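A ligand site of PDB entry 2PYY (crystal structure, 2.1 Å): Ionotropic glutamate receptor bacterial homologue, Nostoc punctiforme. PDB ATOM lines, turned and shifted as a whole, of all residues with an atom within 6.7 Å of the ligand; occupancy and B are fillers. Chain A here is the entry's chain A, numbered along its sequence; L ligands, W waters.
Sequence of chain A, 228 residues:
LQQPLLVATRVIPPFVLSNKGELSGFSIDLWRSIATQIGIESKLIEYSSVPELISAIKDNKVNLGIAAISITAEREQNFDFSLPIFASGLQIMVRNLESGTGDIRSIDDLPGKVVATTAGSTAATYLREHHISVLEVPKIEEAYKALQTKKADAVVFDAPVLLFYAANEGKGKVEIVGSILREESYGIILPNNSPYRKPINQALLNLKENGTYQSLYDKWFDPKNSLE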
ATOM      1  N   ARG A  10      -9.360  -4.548 -30.478  1.00  0.00           N
ATOM      2  CA  ARG A  10     -10.049  -5.437 -31.398  1.00  0.00           C
ATOM      3  C   ARG A  10     -10.891  -4.527 -32.263  1.00  0.00           C
ATOM      4  O   ARG A  10     -11.534  -3.596 -31.760  1.00  0.00           O
ATOM      5  CB  ARG A  10     -10.920  -6.409 -30.585  1.00  0.00           C
ATOM      6  CG  ARG A  10     -11.561  -7.522 -31.371  1.00  0.00           C
ATOM      7  CD  ARG A  10     -12.905  -7.108 -31.917  1.00  0.00           C
ATOM      8  NE  ARG A  10     -13.537  -8.190 -32.658  1.00  0.00           N
ATOM      9  CZ  ARG A  10     -13.773  -9.399 -32.161  1.00  0.00           C
ATOM     10  NH1 ARG A  10     -13.430  -9.692 -30.909  1.00  0.00           N
ATOM     11  NH2 ARG A  10     -14.361 -10.331 -32.909  1.00  0.00           N
ATOM     12  N   VAL A  11     -10.872  -4.768 -33.571  1.00  0.00           N
ATOM     13  CA  VAL A  11     -11.635  -3.939 -34.490  1.00  0.00           C
ATOM     14  C   VAL A  11     -13.112  -4.274 -34.385  1.00  0.00           C
ATOM     15  O   VAL A  11     -13.523  -5.409 -34.618  1.00  0.00           O
ATOM     16  CB  VAL A  11     -11.152  -4.125 -35.927  1.00  0.00           C
ATOM     17  CG1 VAL A  11     -12.002  -3.280 -36.876  1.00  0.00           C
ATOM     18  CG2 VAL A  11      -9.695  -3.711 -36.034  1.00  0.00           C
ATOM     19  N   ILE A  12     -13.912  -3.280 -34.011  1.00  0.00           N
ATOM     20  CA  ILE A  12     -15.343  -3.459 -33.851  1.00  0.00           C
ATOM     21  C   ILE A  12     -16.048  -2.085 -33.835  1.00  0.00           C
ATOM     22  O   ILE A  12     -16.246  -1.481 -32.787  1.00  0.00           O
ATOM     23  CB  ILE A  12     -15.630  -4.234 -32.543  1.00  0.00           C
ATOM     24  CG1 ILE A  12     -17.130  -4.416 -32.353  1.00  0.00           C
ATOM     25  CG2 ILE A  12     -15.005  -3.498 -31.347  1.00  0.00           C
ATOM     26  CD1 ILE A  12     -17.485  -5.349 -31.183  1.00  0.00           C
ATOM     27  N   SER A  48      -7.706 -10.791 -32.879  1.00  0.00           N
ATOM     28  CA  SER A  48      -8.823 -11.311 -33.667  1.00  0.00           C
ATOM     29  C   SER A  48     -10.129 -11.602 -32.936  1.00  0.00           C
ATOM     30  O   SER A  48     -11.187 -11.671 -33.564  1.00  0.00           O
ATOM     31  CB  SER A  48      -8.376 -12.598 -34.372  1.00  0.00           C
ATOM     32  OG  SER A  48      -7.138 -12.405 -35.026  1.00  0.00           O
ATOM     33  N   SER A  49     -10.066 -11.799 -31.632  1.00  0.00           N
ATOM     34  CA  SER A  49     -11.275 -12.096 -30.863  1.00  0.00           C
ATOM     35  C   SER A  49     -11.062 -11.689 -29.419  1.00  0.00           C
ATOM     36  O   SER A  49      -9.934 -11.482 -28.988  1.00  0.00           O
ATOM     37  CB  SER A  49     -11.583 -13.597 -30.913  1.00  0.00           C
ATOM     38  OG  SER A  49     -10.646 -14.329 -30.163  1.00  0.00           O
ATOM     39  N   VAL A  50     -12.164 -11.564 -28.685  1.00  0.00           N
ATOM     40  CA  VAL A  50     -12.075 -11.180 -27.292  1.00  0.00           C
ATOM     41  C   VAL A  50     -11.273 -12.196 -26.503  1.00  0.00           C
ATOM     42  O   VAL A  50     -10.387 -11.825 -25.721  1.00  0.00           O
ATOM     43  CB  VAL A  50     -13.469 -11.019 -26.661  1.00  0.00           C
ATOM     44  CG1 VAL A  50     -13.346 -10.641 -25.186  1.00  0.00           C
ATOM     45  CG2 VAL A  50     -14.250  -9.962 -27.421  1.00  0.00           C
ATOM     46  N   PRO A  51     -11.566 -13.504 -26.668  1.00  0.00           N
ATOM     47  CA  PRO A  51     -10.799 -14.498 -25.908  1.00  0.00           C
ATOM     48  C   PRO A  51      -9.303 -14.429 -26.196  1.00  0.00           C
ATOM     49  O   PRO A  51      -8.484 -14.713 -25.318  1.00  0.00           O
ATOM     50  CB  PRO A  51     -11.434 -15.831 -26.329  1.00  0.00           C
ATOM     51  CG  PRO A  51     -12.046 -15.523 -27.673  1.00  0.00           C
ATOM     52  CD  PRO A  51     -12.617 -14.143 -27.473  1.00  0.00           C
ATOM     53  N   ALA A  67     -11.833  -2.007 -26.246  1.00  0.00           N
ATOM     54  CA  ALA A  67     -12.557  -2.119 -27.506  1.00  0.00           C
ATOM     55  C   ALA A  67     -14.027  -2.072 -27.114  1.00  0.00           C
ATOM     56  O   ALA A  67     -14.525  -1.023 -26.702  1.00  0.00           O
ATOM     57  CB  ALA A  67     -12.213  -3.455 -28.209  1.00  0.00           C
ATOM     58  N   ALA A  68     -14.720  -3.199 -27.243  1.00  0.00           N
ATOM     59  CA  ALA A  68     -16.130  -3.297 -26.851  1.00  0.00           C
ATOM     60  C   ALA A  68     -16.205  -4.534 -25.953  1.00  0.00           C
ATOM     61  O   ALA A  68     -16.979  -5.472 -26.200  1.00  0.00           O
ATOM     62  CB  ALA A  68     -17.020  -3.473 -28.095  1.00  0.00           C
ATOM     63  N   ILE A  69     -15.387  -4.516 -24.901  1.00  0.00           N
ATOM     64  CA  ILE A  69     -15.263  -5.623 -23.953  1.00  0.00           C
ATOM     65  C   ILE A  69     -16.261  -5.629 -22.785  1.00  0.00           C
ATOM     66  O   ILE A  69     -16.153  -4.822 -21.862  1.00  0.00           O
ATOM     67  CB  ILE A  69     -13.838  -5.649 -23.360  1.00  0.00           C
ATOM     68  CG1 ILE A  69     -12.811  -5.521 -24.507  1.00  0.00           C
ATOM     69  CG2 ILE A  69     -13.622  -6.958 -22.579  1.00  0.00           C
ATOM     70  CD1 ILE A  69     -11.337  -5.404 -24.031  1.00  0.00           C
ATOM     71  N   SER A  70     -17.207  -6.573 -22.814  1.00  0.00           N
ATOM     72  CA  SER A  70     -18.199  -6.692 -21.780  1.00  0.00           C
ATOM     73  C   SER A  70     -17.651  -7.095 -20.425  1.00  0.00           C
ATOM     74  O   SER A  70     -16.781  -7.964 -20.323  1.00  0.00           O
ATOM     75  CB  SER A  70     -19.276  -7.695 -22.188  1.00  0.00           C
ATOM     76  OG  SER A  70     -19.963  -7.239 -23.345  1.00  0.00           O
ATOM     77  N   ILE A  71     -18.169  -6.437 -19.384  1.00  0.00           N
ATOM     78  CA  ILE A  71     -17.778  -6.741 -18.015  1.00  0.00           C
ATOM     79  C   ILE A  71     -18.763  -7.826 -17.561  1.00  0.00           C
ATOM     80  O   ILE A  71     -19.970  -7.588 -17.471  1.00  0.00           O
ATOM     81  CB  ILE A  71     -17.906  -5.504 -17.123  1.00  0.00           C
ATOM     82  CG1 ILE A  71     -16.951  -4.404 -17.638  1.00  0.00           C
ATOM     83  CG2 ILE A  71     -17.598  -5.867 -15.673  1.00  0.00           C
ATOM     84  CD1 ILE A  71     -16.971  -3.135 -16.823  1.00  0.00           C
ATOM     85  N   THR A  72     -18.236  -9.017 -17.282  1.00  0.00           N
ATOM     86  CA  THR A  72     -19.024 -10.186 -16.839  1.00  0.00           C
ATOM     87  C   THR A  72     -18.375 -10.789 -15.584  1.00  0.00           C
ATOM     88  O   THR A  72     -17.199 -10.549 -15.330  1.00  0.00           O
ATOM     89  CB  THR A  72     -19.047 -11.302 -17.915  1.00  0.00           C
ATOM     90  OG1 THR A  72     -17.745 -11.883 -18.038  1.00  0.00           O
ATOM     91  CG2 THR A  72     -19.465 -10.760 -19.265  1.00  0.00           C
ATOM     92  N   ARG A  75     -15.264 -12.980 -16.240  1.00  0.00           N
ATOM     93  CA  ARG A  75     -14.041 -12.215 -16.525  1.00  0.00           C
ATOM     94  C   ARG A  75     -13.489 -11.514 -15.289  1.00  0.00           C
ATOM     95  O   ARG A  75     -12.271 -11.514 -15.062  1.00  0.00           O
ATOM     96  CB  ARG A  75     -14.307 -11.216 -17.662  1.00  0.00           C
ATOM     97  CG  ARG A  75     -14.498 -11.910 -19.025  1.00  0.00           C
ATOM     98  CD  ARG A  75     -15.032 -10.952 -20.106  1.00  0.00           C
ATOM     99  NE  ARG A  75     -15.327 -11.649 -21.359  1.00  0.00           N
ATOM    100  CZ  ARG A  75     -15.876 -11.071 -22.432  1.00  0.00           C
ATOM    101  NH1 ARG A  75     -16.179  -9.775 -22.399  1.00  0.00           N
ATOM    102  NH2 ARG A  75     -16.113 -11.773 -23.544  1.00  0.00           N
ATOM    103  N   SER A  88     -23.993  -0.963 -22.680  1.00  0.00           N
ATOM    104  CA  SER A  88     -24.386  -1.743 -23.841  1.00  0.00           C
ATOM    105  C   SER A  88     -25.373  -2.847 -23.476  1.00  0.00           C
ATOM    106  O   SER A  88     -25.996  -2.803 -22.411  1.00  0.00           O
ATOM    107  CB  SER A  88     -23.141  -2.345 -24.501  1.00  0.00           C
ATOM    108  OG  SER A  88     -23.454  -3.050 -25.690  1.00  0.00           O
ATOM    109  N   LEU A  90     -27.145  -6.971 -25.184  1.00  0.00           N
ATOM    110  CA  LEU A  90     -27.447  -7.868 -26.301  1.00  0.00           C
ATOM    111  C   LEU A  90     -28.772  -7.524 -26.958  1.00  0.00           C
ATOM    112  O   LEU A  90     -29.761  -7.217 -26.284  1.00  0.00           O
ATOM    113  CB  LEU A  90     -27.500  -9.314 -25.797  1.00  0.00           C
ATOM    114  CG  LEU A  90     -26.210  -9.774 -25.130  1.00  0.00           C
ATOM    115  CD1 LEU A  90     -26.355 -11.182 -24.594  1.00  0.00           C
ATOM    116  CD2 LEU A  90     -25.078  -9.711 -26.165  1.00  0.00           C
ATOM    117  N   THR A 118     -20.484 -13.547 -33.184  1.00  0.00           N
ATOM    118  CA  THR A 118     -19.051 -13.794 -33.228  1.00  0.00           C
ATOM    119  C   THR A 118     -18.671 -14.869 -32.242  1.00  0.00           C
ATOM    120  O   THR A 118     -19.323 -15.014 -31.199  1.00  0.00           O
ATOM    121  CB  THR A 118     -18.243 -12.524 -32.908  1.00  0.00           C
ATOM    122  OG1 THR A 118     -18.446 -12.165 -31.532  1.00  0.00           O
ATOM    123  CG2 THR A 118     -18.695 -11.374 -33.793  1.00  0.00           C
ATOM    124  N   ALA A 119     -17.627 -15.637 -32.547  1.00  0.00           N
ATOM    125  CA  ALA A 119     -17.174 -16.692 -31.629  1.00  0.00           C
ATOM    126  C   ALA A 119     -16.483 -16.037 -30.427  1.00  0.00           C
ATOM    127  O   ALA A 119     -15.830 -15.013 -30.572  1.00  0.00           O
ATOM    128  CB  ALA A 119     -16.205 -17.662 -32.367  1.00  0.00           C
ATOM    129  N   GLY A 120     -16.640 -16.603 -29.232  1.00  0.00           N
ATOM    130  CA  GLY A 120     -15.964 -16.043 -28.080  1.00  0.00           C
ATOM    131  C   GLY A 120     -16.647 -14.867 -27.412  1.00  0.00           C
ATOM    132  O   GLY A 120     -16.128 -14.339 -26.421  1.00  0.00           O
ATOM    133  N   SER A 121     -17.800 -14.444 -27.926  1.00  0.00           N
ATOM    134  CA  SER A 121     -18.506 -13.290 -27.353  1.00  0.00           C
ATOM    135  C   SER A 121     -19.461 -13.653 -26.238  1.00  0.00           C
ATOM    136  O   SER A 121     -19.742 -14.812 -25.978  1.00  0.00           O
ATOM    137  CB  SER A 121     -19.305 -12.541 -28.420  1.00  0.00           C
ATOM    138  OG  SER A 121     -20.201 -13.414 -29.072  1.00  0.00           O
ATOM    139  N   THR A 122     -19.970 -12.625 -25.580  1.00  0.00           N
ATOM    140  CA  THR A 122     -20.938 -12.832 -24.534  1.00  0.00           C
ATOM    141  C   THR A 122     -22.232 -13.283 -25.215  1.00  0.00           C
ATOM    142  O   THR A 122     -22.989 -14.063 -24.640  1.00  0.00           O
ATOM    143  CB  THR A 122     -21.173 -11.530 -23.729  1.00  0.00           C
ATOM    144  OG1 THR A 122     -21.450 -10.447 -24.620  1.00  0.00           O
ATOM    145  CG2 THR A 122     -19.906 -11.200 -22.913  1.00  0.00           C
ATOM    146  N   ALA A 123     -22.477 -12.787 -26.432  1.00  0.00           N
ATOM    147  CA  ALA A 123     -23.676 -13.196 -27.163  1.00  0.00           C
ATOM    148  C   ALA A 123     -23.630 -14.716 -27.323  1.00  0.00           C
ATOM    149  O   ALA A 123     -24.619 -15.417 -27.044  1.00  0.00           O
ATOM    150  CB  ALA A 123     -23.717 -12.500 -28.539  1.00  0.00           C
ATOM    151  N   PRO A 138     -15.785 -16.281 -36.849  1.00  0.00           N
ATOM    152  CA  PRO A 138     -14.629 -15.537 -36.334  1.00  0.00           C
ATOM    153  C   PRO A 138     -14.736 -14.035 -36.586  1.00  0.00           C
ATOM    154  O   PRO A 138     -14.134 -13.241 -35.858  1.00  0.00           O
ATOM    155  CB  PRO A 138     -13.445 -16.189 -37.043  1.00  0.00           C
ATOM    156  CG  PRO A 138     -14.039 -16.724 -38.316  1.00  0.00           C
ATOM    157  CD  PRO A 138     -15.372 -17.257 -37.879  1.00  0.00           C
ATOM    158  N   ILE A 140     -17.586 -10.865 -37.258  1.00  0.00           N
ATOM    159  CA  ILE A 140     -18.987 -10.431 -37.240  1.00  0.00           C
ATOM    160  C   ILE A 140     -19.570 -10.234 -38.634  1.00  0.00           C
ATOM    161  O   ILE A 140     -20.753 -10.480 -38.858  1.00  0.00           O
ATOM    162  CB  ILE A 140     -19.171  -9.113 -36.468  1.00  0.00           C
ATOM    163  CG1 ILE A 140     -20.652  -8.832 -36.245  1.00  0.00           C
ATOM    164  CG2 ILE A 140     -18.563  -7.956 -37.264  1.00  0.00           C
ATOM    165  CD1 ILE A 140     -21.343  -9.825 -35.341  1.00  0.00           C
ATOM    166  N   PHE A 157     -26.167  -9.734 -31.018  1.00  0.00           N
ATOM    167  CA  PHE A 157     -24.871  -9.119 -30.747  1.00  0.00           C
ATOM    168  C   PHE A 157     -25.133  -7.831 -30.005  1.00  0.00           C
ATOM    169  O   PHE A 157     -26.282  -7.515 -29.667  1.00  0.00           O
ATOM    170  CB  PHE A 157     -24.136  -8.875 -32.070  1.00  0.00           C
ATOM    171  CG  PHE A 157     -22.628  -8.766 -31.915  1.00  0.00           C
ATOM    172  CD1 PHE A 157     -21.935  -9.686 -31.133  1.00  0.00           C
ATOM    173  CD2 PHE A 157     -21.917  -7.743 -32.536  1.00  0.00           C
ATOM    174  CE1 PHE A 157     -20.536  -9.571 -30.956  1.00  0.00           C
ATOM    175  CE2 PHE A 157     -20.532  -7.627 -32.376  1.00  0.00           C
ATOM    176  CZ  PHE A 157     -19.833  -8.544 -31.581  1.00  0.00           C
ATOM    177  N   ASP A 158     -24.062  -7.098 -29.720  1.00  0.00           N
ATOM    178  CA  ASP A 158     -24.129  -5.833 -28.971  1.00  0.00           C
ATOM    179  C   ASP A 158     -24.982  -4.774 -29.692  1.00  0.00           C
ATOM    180  O   ASP A 158     -24.733  -4.449 -30.855  1.00  0.00           O
ATOM    181  CB  ASP A 158     -22.712  -5.291 -28.759  1.00  0.00           C
ATOM    182  CG  ASP A 158     -21.784  -6.311 -28.119  1.00  0.00           C
ATOM    183  OD1 ASP A 158     -21.773  -7.486 -28.566  1.00  0.00           O
ATOM    184  OD2 ASP A 158     -21.043  -5.944 -27.202  1.00  0.00           O
ATOM    185  N   GLU A 184     -25.358  -4.968 -20.547  1.00  0.00           N
ATOM    186  CA  GLU A 184     -23.920  -5.203 -20.313  1.00  0.00           C
ATOM    187  C   GLU A 184     -23.183  -3.873 -20.440  1.00  0.00           C
ATOM    188  O   GLU A 184     -23.472  -3.071 -21.331  1.00  0.00           O
ATOM    189  CB  GLU A 184     -23.297  -6.159 -21.337  1.00  0.00           C
ATOM    190  CG  GLU A 184     -23.955  -7.522 -21.496  1.00  0.00           C
ATOM    191  CD  GLU A 184     -23.058  -8.524 -22.235  1.00  0.00           C
ATOM    192  OE1 GLU A 184     -22.449  -8.159 -23.263  1.00  0.00           O
ATOM    193  OE2 GLU A 184     -22.980  -9.690 -21.806  1.00  0.00           O
ATOM    194  N   TYR A 186     -19.402  -1.845 -20.912  1.00  0.00           N
ATOM    195  CA  TYR A 186     -18.067  -2.074 -21.446  1.00  0.00           C
ATOM    196  C   TYR A 186     -17.080  -1.462 -20.473  1.00  0.00           C
ATOM    197  O   TYR A 186     -17.372  -0.450 -19.819  1.00  0.00           O
ATOM    198  CB  TYR A 186     -17.868  -1.364 -22.788  1.00  0.00           C
ATOM    199  CG  TYR A 186     -18.685  -1.864 -23.956  1.00  0.00           C
ATOM    200  CD1 TYR A 186     -19.227  -3.161 -23.967  1.00  0.00           C
ATOM    201  CD2 TYR A 186     -18.863  -1.067 -25.090  1.00  0.00           C
ATOM    202  CE1 TYR A 186     -19.913  -3.641 -25.079  1.00  0.00           C
ATOM    203  CE2 TYR A 186     -19.542  -1.526 -26.202  1.00  0.00           C
ATOM    204  CZ  TYR A 186     -20.068  -2.810 -26.193  1.00  0.00           C
ATOM    205  OH  TYR A 186     -20.733  -3.264 -27.303  1.00  0.00           O
HETATM  206  N1  LIG L   1     -18.905  -7.170 -26.037  1.00  0.00           N
HETATM  207  C1  LIG L   1     -18.538  -8.484 -26.646  1.00  0.00           C
HETATM  208  C2  LIG L   1     -17.722  -9.307 -25.648  1.00  0.00           C
HETATM  209  O1  LIG L   1     -17.010  -8.693 -24.823  1.00  0.00           O
HETATM  210  C3  LIG L   1     -17.714  -8.267 -27.930  1.00  0.00           C
HETATM  211  C4  LIG L   1     -17.424  -9.565 -28.682  1.00  0.00           C
HETATM  212  C5  LIG L   1     -16.515  -9.371 -29.880  1.00  0.00           C
HETATM  213  O2  LIG L   1     -16.308 -10.360 -30.621  1.00  0.00           O
HETATM  214  O3  LIG L   1     -16.005  -8.256 -30.080  1.00  0.00           O
HETATM  215  O4  LIG L   1     -17.791 -10.551 -25.704  1.00  0.00           O
HETATM  216  O   HOH W   1     -14.957 -12.470 -29.593  1.00  0.00           O
HETATM  217  O   HOH W   2     -14.629  -6.030 -28.242  1.00  0.00           O
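Water W1 lies within hydrogen-bond range of O2 of the ligand, O of Ala 119, N of Val 50 and NH1 of Arg 10.
Water W2 bridges N of Ala 68 (3.0 Å) and O3 of the ligand (3.2 Å).
O of Thr 118 is in hydrogen-bond range of OG of Ser 121, 2.8 Å away.
The side-chain hydroxyl (OH) of Tyr 186 lies within hydrogen-bond range of the side-chain carboxylate (OD2) of Asp 158 (2.7 Å).
The side-chain hydroxyl (OG1) of Thr 122 is in hydrogen-bond range of the side-chain carboxylate (OE1) of Glu 184, at 2.8 Å.
The side-chain carboxylate of Glu 184 lies within hydrogen-bond range of the side-chain hydroxyl of Ser 70 (2.7 Å).
OH of Tyr 186 lies within hydrogen-bond range of OG of Ser 88 (3.2 Å).
The backbone carbonyl oxygen of Ser 70 is in hydrogen-bond range of the guanidinium group of Arg 75, 2.8 Å away.
The backbone NH of Arg 75 sits at hydrogen-bond distance from the side-chain hydroxyl of Thr 72 (3.3 Å).
The guanidinium group (NH1) of Arg 75 is in salt-bridge range of an oxygen (O1) of the ligand, 2.8 Å away.
The backbone NH (N) of Ser 70 is in hydrogen-bond range of an oxygen (O1) of the ligand (2.9 Å).
The guanidinium group of Arg 10 lies within salt-bridge range of an oxygen (O2) of the ligand, at 3.0 Å.
A nitrogen (N1) of the ligand sits at hydrogen-bond distance from the side-chain hydroxyl of Ser 70.
N of Thr 122 is in hydrogen-bond range of O4 of the ligand, 3.0 Å away.
OD2 of Asp 158 lies within salt-bridge range of N1 of the ligand (2.7 Å).
The backbone carbonyl oxygen of Ala 68 sits at hydrogen-bond distance from a nitrogen (N1) of the ligand.
The side-chain hydroxyl (OG1) of Thr 118 is in hydrogen-bond range of an oxygen (O2) of the ligand (2.9 Å).
Ile 12 touches the ligand (CD1 to O3, 3.4 Å).
Val 50 touches the ligand (CG2 to C5, 3.4 Å).
Ile 69 touches the ligand.
Ser 121 touches the ligand.
Phe 157 touches the ligand (CZ to C5, 3.8 Å).
Tyr 186 touches the ligand (CE1 to N1, 3.8 Å).
Hydrophobic or aromatic side chains within 4 Å of the ligand: Ile 12, Val 50, Phe 157 and Tyr 186.
13 residues have an atom within 4 Å of the ligand: Arg 10, Ile 12, Val 50, Ala 68, Ile 69, Ser 70, Arg 75, Thr 118, Ser 121, Thr 122, Phe 157, Asp 158 and Tyr 186.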
